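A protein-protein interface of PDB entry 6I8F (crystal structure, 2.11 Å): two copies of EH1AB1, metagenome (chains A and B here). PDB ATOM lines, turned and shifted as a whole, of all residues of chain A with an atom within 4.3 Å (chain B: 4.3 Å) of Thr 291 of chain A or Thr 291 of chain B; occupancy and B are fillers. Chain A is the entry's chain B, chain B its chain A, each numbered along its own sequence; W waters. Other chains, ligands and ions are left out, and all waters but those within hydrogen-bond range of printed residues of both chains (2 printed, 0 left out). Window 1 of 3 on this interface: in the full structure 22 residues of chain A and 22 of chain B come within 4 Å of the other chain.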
ATOM      1  N   ALA A 262      12.434 -19.434 -37.309  1.00  0.00           N
ATOM      2  CA  ALA A 262      11.175 -19.089 -36.677  1.00  0.00           C
ATOM      3  C   ALA A 262      11.221 -19.269 -35.151  1.00  0.00           C
ATOM      4  O   ALA A 262      11.861 -20.165 -34.604  1.00  0.00           O
ATOM      5  CB  ALA A 262      10.093 -19.943 -37.267  1.00  0.00           C
ATOM      6  N   PHE A 263      10.472 -18.402 -34.480  1.00  0.00           N
ATOM      7  CA  PHE A 263      10.024 -18.593 -33.133  1.00  0.00           C
ATOM      8  C   PHE A 263       8.498 -18.637 -33.163  1.00  0.00           C
ATOM      9  O   PHE A 263       7.878 -17.671 -33.602  1.00  0.00           O
ATOM     10  CB  PHE A 263      10.502 -17.446 -32.244  1.00  0.00           C
ATOM     11  CG  PHE A 263       9.956 -17.473 -30.837  1.00  0.00           C
ATOM     12  CD1 PHE A 263      10.585 -18.207 -29.850  1.00  0.00           C
ATOM     13  CD2 PHE A 263       8.821 -16.745 -30.496  1.00  0.00           C
ATOM     14  CE1 PHE A 263      10.084 -18.228 -28.552  1.00  0.00           C
ATOM     15  CE2 PHE A 263       8.334 -16.753 -29.199  1.00  0.00           C
ATOM     16  CZ  PHE A 263       8.958 -17.501 -28.227  1.00  0.00           C
ATOM     17  N   VAL A 264       7.922 -19.754 -32.705  1.00  0.00           N
ATOM     18  CA  VAL A 264       6.499 -19.956 -32.677  1.00  0.00           C
ATOM     19  C   VAL A 264       6.044 -20.220 -31.235  1.00  0.00           C
ATOM     20  O   VAL A 264       6.491 -21.186 -30.586  1.00  0.00           O
ATOM     21  CB  VAL A 264       6.098 -21.116 -33.604  1.00  0.00           C
ATOM     22  CG1 VAL A 264       4.586 -21.263 -33.686  1.00  0.00           C
ATOM     23  CG2 VAL A 264       6.694 -20.953 -34.996  1.00  0.00           C
ATOM     24  N   THR A 290      13.828 -23.782 -36.048  1.00  0.00           N
ATOM     25  CA  THR A 290      12.548 -23.441 -35.492  1.00  0.00           C
ATOM     26  C   THR A 290      12.569 -23.644 -33.974  1.00  0.00           C
ATOM     27  O   THR A 290      12.928 -24.712 -33.497  1.00  0.00           O
ATOM     28  CB  THR A 290      11.427 -24.297 -36.094  1.00  0.00           C
ATOM     29  OG1 THR A 290      11.502 -24.218 -37.517  1.00  0.00           O
ATOM     30  CG2 THR A 290      10.047 -23.873 -35.646  1.00  0.00           C
ATOM     31  N   THR A 291      12.131 -22.611 -33.250  1.00  0.00           N
ATOM     32  CA  THR A 291      11.894 -22.662 -31.822  1.00  0.00           C
ATOM     33  C   THR A 291      10.381 -22.626 -31.587  1.00  0.00           C
ATOM     34  O   THR A 291       9.706 -21.681 -32.017  1.00  0.00           O
ATOM     35  CB  THR A 291      12.599 -21.508 -31.095  1.00  0.00           C
ATOM     36  OG1 THR A 291      13.987 -21.547 -31.429  1.00  0.00           O
ATOM     37  CG2 THR A 291      12.445 -21.560 -29.587  1.00  0.00           C
ATOM     38  N   TYR A 292       9.869 -23.642 -30.887  1.00  0.00           N
ATOM     39  CA  TYR A 292       8.466 -23.731 -30.517  1.00  0.00           C
ATOM     40  C   TYR A 292       8.345 -23.701 -28.995  1.00  0.00           C
ATOM     41  O   TYR A 292       9.106 -24.381 -28.310  1.00  0.00           O
ATOM     42  CB  TYR A 292       7.817 -25.019 -31.037  1.00  0.00           C
ATOM     43  CG  TYR A 292       6.438 -25.221 -30.466  1.00  0.00           C
ATOM     44  CD1 TYR A 292       5.358 -24.487 -30.936  1.00  0.00           C
ATOM     45  CD2 TYR A 292       6.213 -26.095 -29.411  1.00  0.00           C
ATOM     46  CE1 TYR A 292       4.094 -24.623 -30.382  1.00  0.00           C
ATOM     47  CE2 TYR A 292       4.954 -26.239 -28.849  1.00  0.00           C
ATOM     48  CZ  TYR A 292       3.885 -25.508 -29.341  1.00  0.00           C
ATOM     49  OH  TYR A 292       2.633 -25.640 -28.787  1.00  0.00           O
ATOM     50  N   VAL A 293       7.375 -22.942 -28.478  1.00  0.00           N
ATOM     51  CA  VAL A 293       7.086 -22.947 -27.043  1.00  0.00           C
ATOM     52  C   VAL A 293       5.572 -22.897 -26.824  1.00  0.00           C
ATOM     53  O   VAL A 293       4.869 -22.120 -27.451  1.00  0.00           O
ATOM     54  CB  VAL A 293       7.795 -21.819 -26.264  1.00  0.00           C
ATOM     55  CG1 VAL A 293       7.493 -20.436 -26.803  1.00  0.00           C
ATOM     56  CG2 VAL A 293       7.466 -21.877 -24.782  1.00  0.00           C
ATOM     57  N   GLU A 318      10.888 -13.933 -23.688  1.00  0.00           N
ATOM     58  CA  GLU A 318      11.382 -15.109 -24.381  1.00  0.00           C
ATOM     59  C   GLU A 318      11.471 -14.827 -25.884  1.00  0.00           C
ATOM     60  O   GLU A 318      12.459 -15.153 -26.529  1.00  0.00           O
ATOM     61  CB  GLU A 318      10.514 -16.339 -24.134  1.00  0.00           C
ATOM     62  CG  GLU A 318      11.147 -17.577 -24.756  1.00  0.00           C
ATOM     63  CD  GLU A 318      10.506 -18.915 -24.448  1.00  0.00           C
ATOM     64  OE1 GLU A 318       9.496 -18.947 -23.689  1.00  0.00           O
ATOM     65  OE2 GLU A 318      11.027 -19.924 -24.974  1.00  0.00           O
ATOM     66  N   VAL A 322      15.083 -14.798 -27.845  1.00  0.00           N
ATOM     67  CA  VAL A 322      15.377 -15.754 -28.907  1.00  0.00           C
ATOM     68  C   VAL A 322      15.756 -14.995 -30.190  1.00  0.00           C
ATOM     69  O   VAL A 322      16.735 -15.356 -30.874  1.00  0.00           O
ATOM     70  CB  VAL A 322      14.195 -16.707 -29.138  1.00  0.00           C
ATOM     71  CG1 VAL A 322      14.366 -17.531 -30.400  1.00  0.00           C
ATOM     72  CG2 VAL A 322      13.978 -17.597 -27.935  1.00  0.00           C
ATOM     73  N   ALA B 262      11.162 -26.343 -19.359  1.00  0.00           N
ATOM     74  CA  ALA B 262      12.286 -26.921 -20.037  1.00  0.00           C
ATOM     75  C   ALA B 262      12.611 -26.126 -21.300  1.00  0.00           C
ATOM     76  O   ALA B 262      11.744 -25.484 -21.883  1.00  0.00           O
ATOM     77  CB  ALA B 262      11.969 -28.364 -20.380  1.00  0.00           C
ATOM     78  N   PHE B 263      13.895 -26.176 -21.663  1.00  0.00           N
ATOM     79  CA  PHE B 263      14.409 -25.857 -22.967  1.00  0.00           C
ATOM     80  C   PHE B 263      15.056 -27.140 -23.499  1.00  0.00           C
ATOM     81  O   PHE B 263      15.947 -27.676 -22.844  1.00  0.00           O
ATOM     82  CB  PHE B 263      15.408 -24.704 -22.868  1.00  0.00           C
ATOM     83  CG  PHE B 263      16.140 -24.379 -24.142  1.00  0.00           C
ATOM     84  CD1 PHE B 263      15.594 -23.514 -25.074  1.00  0.00           C
ATOM     85  CD2 PHE B 263      17.380 -24.918 -24.409  1.00  0.00           C
ATOM     86  CE1 PHE B 263      16.270 -23.201 -26.241  1.00  0.00           C
ATOM     87  CE2 PHE B 263      18.048 -24.625 -25.588  1.00  0.00           C
ATOM     88  CZ  PHE B 263      17.499 -23.750 -26.491  1.00  0.00           C
ATOM     89  N   VAL B 264      14.598 -27.629 -24.655  1.00  0.00           N
ATOM     90  CA  VAL B 264      15.115 -28.871 -25.250  1.00  0.00           C
ATOM     91  C   VAL B 264      15.637 -28.539 -26.653  1.00  0.00           C
ATOM     92  O   VAL B 264      14.898 -28.020 -27.497  1.00  0.00           O
ATOM     93  CB  VAL B 264      14.038 -29.975 -25.289  1.00  0.00           C
ATOM     94  CG1 VAL B 264      14.610 -31.279 -25.814  1.00  0.00           C
ATOM     95  CG2 VAL B 264      13.378 -30.197 -23.934  1.00  0.00           C
ATOM     96  N   THR B 290       7.349 -25.676 -22.270  1.00  0.00           N
ATOM     97  CA  THR B 290       8.441 -26.319 -22.941  1.00  0.00           C
ATOM     98  C   THR B 290       8.804 -25.504 -24.177  1.00  0.00           C
ATOM     99  O   THR B 290       7.944 -25.230 -24.997  1.00  0.00           O
ATOM    100  CB  THR B 290       8.089 -27.757 -23.339  1.00  0.00           C
ATOM    101  OG1 THR B 290       7.552 -28.408 -22.189  1.00  0.00           O
ATOM    102  CG2 THR B 290       9.274 -28.524 -23.887  1.00  0.00           C
ATOM    103  N   THR B 291      10.081 -25.156 -24.292  1.00  0.00           N
ATOM    104  CA  THR B 291      10.625 -24.564 -25.486  1.00  0.00           C
ATOM    105  C   THR B 291      11.492 -25.604 -26.200  1.00  0.00           C
ATOM    106  O   THR B 291      12.467 -26.073 -25.625  1.00  0.00           O
ATOM    107  CB  THR B 291      11.467 -23.335 -25.139  1.00  0.00           C
ATOM    108  OG1 THR B 291      10.675 -22.439 -24.356  1.00  0.00           O
ATOM    109  CG2 THR B 291      12.003 -22.635 -26.367  1.00  0.00           C
ATOM    110  N   TYR B 292      11.129 -25.955 -27.435  1.00  0.00           N
ATOM    111  CA  TYR B 292      11.859 -26.926 -28.235  1.00  0.00           C
ATOM    112  C   TYR B 292      12.490 -26.215 -29.434  1.00  0.00           C
ATOM    113  O   TYR B 292      11.837 -25.409 -30.084  1.00  0.00           O
ATOM    114  CB  TYR B 292      10.950 -28.051 -28.743  1.00  0.00           C
ATOM    115  CG  TYR B 292      11.648 -28.909 -29.765  1.00  0.00           C
ATOM    116  CD1 TYR B 292      12.596 -29.843 -29.374  1.00  0.00           C
ATOM    117  CD2 TYR B 292      11.447 -28.719 -31.120  1.00  0.00           C
ATOM    118  CE1 TYR B 292      13.283 -30.608 -30.304  1.00  0.00           C
ATOM    119  CE2 TYR B 292      12.135 -29.465 -32.065  1.00  0.00           C
ATOM    120  CZ  TYR B 292      13.062 -30.409 -31.658  1.00  0.00           C
ATOM    121  OH  TYR B 292      13.737 -31.154 -32.583  1.00  0.00           O
ATOM    122  N   VAL B 293      13.751 -26.534 -29.728  1.00  0.00           N
ATOM    123  CA  VAL B 293      14.403 -25.989 -30.918  1.00  0.00           C
ATOM    124  C   VAL B 293      15.267 -27.071 -31.565  1.00  0.00           C
ATOM    125  O   VAL B 293      15.948 -27.822 -30.868  1.00  0.00           O
ATOM    126  CB  VAL B 293      15.236 -24.728 -30.616  1.00  0.00           C
ATOM    127  CG1 VAL B 293      16.295 -24.966 -29.553  1.00  0.00           C
ATOM    128  CG2 VAL B 293      15.868 -24.178 -31.888  1.00  0.00           C
ATOM    129  N   GLU B 318      20.958 -18.762 -27.425  1.00  0.00           N
ATOM    130  CA  GLU B 318      19.519 -19.061 -27.363  1.00  0.00           C
ATOM    131  C   GLU B 318      19.156 -19.753 -26.035  1.00  0.00           C
ATOM    132  O   GLU B 318      18.178 -19.401 -25.390  1.00  0.00           O
ATOM    133  CB  GLU B 318      19.064 -19.916 -28.546  1.00  0.00           C
ATOM    134  CG  GLU B 318      17.587 -20.217 -28.479  1.00  0.00           C
ATOM    135  CD  GLU B 318      16.956 -20.859 -29.699  1.00  0.00           C
ATOM    136  OE1 GLU B 318      17.683 -21.195 -30.668  1.00  0.00           O
ATOM    137  OE2 GLU B 318      15.734 -21.040 -29.655  1.00  0.00           O
ATOM    138  N   VAL B 322      16.688 -17.986 -23.263  1.00  0.00           N
ATOM    139  CA  VAL B 322      15.429 -18.556 -22.844  1.00  0.00           C
ATOM    140  C   VAL B 322      15.431 -18.742 -21.315  1.00  0.00           C
ATOM    141  O   VAL B 322      14.426 -18.475 -20.649  1.00  0.00           O
ATOM    142  CB  VAL B 322      15.147 -19.866 -23.600  1.00  0.00           C
ATOM    143  CG1 VAL B 322      13.959 -20.620 -23.024  1.00  0.00           C
ATOM    144  CG2 VAL B 322      14.965 -19.633 -25.091  1.00  0.00           C
HETATM  145  O   HOH W   1      11.850 -18.360 -21.440  1.00  0.00           O
HETATM  146  O   HOH W   2      17.749 -17.836 -31.227  1.00  0.00           O
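Thr 290 of chain A touches Tyr 292 of chain B, and with the chains exchanged Tyr 292 of chain A touches Thr 290 of chain B. Thr 291 of chain A touches Tyr 292 of chain B, and with the chains exchanged Tyr 292 of chain A touches Thr 291 of chain B. Tyr 292 of chain A touches its own counterpart, Tyr 292 of chain B. Glu 318 of chain A touches Val 322 of chain B, and with the chains exchanged Val 322 of chain A touches Glu 318 of chain B. 9 positions are printed for both chains. Of the 15 pairs that touch across the chains among the printed residues, 15 have their exchanged pair printed and touching as well.
The side-chain carboxylate (OE2) of Glu 318 of chain A sits at hydrogen-bond distance from the side-chain hydroxyl (OG1) of Thr 291 of chain B (2.6 Å). The backbone NH (N) of Tyr 292 of chain B sits at hydrogen-bond distance from the backbone carbonyl oxygen (O) of Tyr 292 of chain A, at 2.7 Å. The side-chain carboxylate (OE2) of Glu 318 of chain B sits at hydrogen-bond distance from the side-chain hydroxyl (OG1) of Thr 291 of chain A, at 2.5 Å.
Hydrophobic or aromatic side chains of chain B that line the printed part of chain A: Val 293 and Val 322. Along chain A the printed residues that touch a printed residue of chain B span positions 290 to 322. Among the printed residues, 15 pairs touch across the chains. Among the printed residues, no Asp or Glu carboxylate lies within 4 Å of a Lys or Arg side-chain nitrogen of the other chain.
Water W1 lies within hydrogen-bond range of O of Val 322 of chain B (2.7 Å) and OE1 of Glu 318 of chain A (3.3 Å). Water W2 bridges O of Val 322 of chain A (2.7 Å) and OE1 of Glu 318 of chain B (3.4 Å).
Ala 262 of chain A touches none of the printed residues of chain B. Thr 291 of chain A touches just these residues of chain B: Thr 291 (3.4 Å), Tyr 292 (3.3 Å), Val 293 (3.3 Å) and Glu 318 (2.5 Å). Printed residues of chain B within 4 Å of Glu 318 of chain A: Thr 291 (2.6 Å) and Val 322 (3.6 Å). Of the printed residues of chain A, Thr 290 of chain B touches Tyr 292 and Val 293. Of the printed residues of chain A, Val 293 of chain B touches Thr 290 (3.2 Å) and Thr 291 (3.3 Å).
The backbone carbonyl oxygen (O) of Thr 291 of chain A sits at hydrogen-bond distance from the backbone NH (N) of Val 264 of chain A, at 2.7 Å. The backbone carbonyl oxygen of Val 264 of chain B sits at hydrogen-bond distance from the backbone NH of Val 293 of chain B (2.9 Å). N of Thr 291 of chain B lies within hydrogen-bond range of O of Ala 262 of chain B, 2.9 Å away. The backbone carbonyl oxygen of Val 264 of chain A is in hydrogen-bond range of the backbone NH of Val 293 of chain A (2.9 Å). The backbone carbonyl oxygen of Thr 291 of chain B is in hydrogen-bond range of the backbone NH of Val 264 of chain B (2.8 Å). The backbone NH of Thr 291 of chain A sits at hydrogen-bond distance from the backbone carbonyl oxygen of Ala 262 of chain A (2.8 Å).
Val 293 of chain B touches Thr 290 of chain A. Thr 291 of chain B touches Thr 291 of chain A (CG2 to CG2, 3.4 Å). O of Tyr 292 of chain B touches CA of Thr 291 of chain A, at 3.3 Å. Val 293 of chain B touches Thr 291 of chain A (CG2 to OG1, 3.3 Å). O of Tyr 292 of chain A touches O of Thr 290 of chain B, at 3.6 Å. Val 293 of chain A touches Thr 290 of chain B. Thr 291 of chain B touches Val 293 of chain A (OG1 to CG2, 3.3 Å). Glu 318 of chain A touches Val 322 of chain B. Val 322 of chain A touches Glu 318 of chain B. Val 322 of chain A touches Val 322 of chain B.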
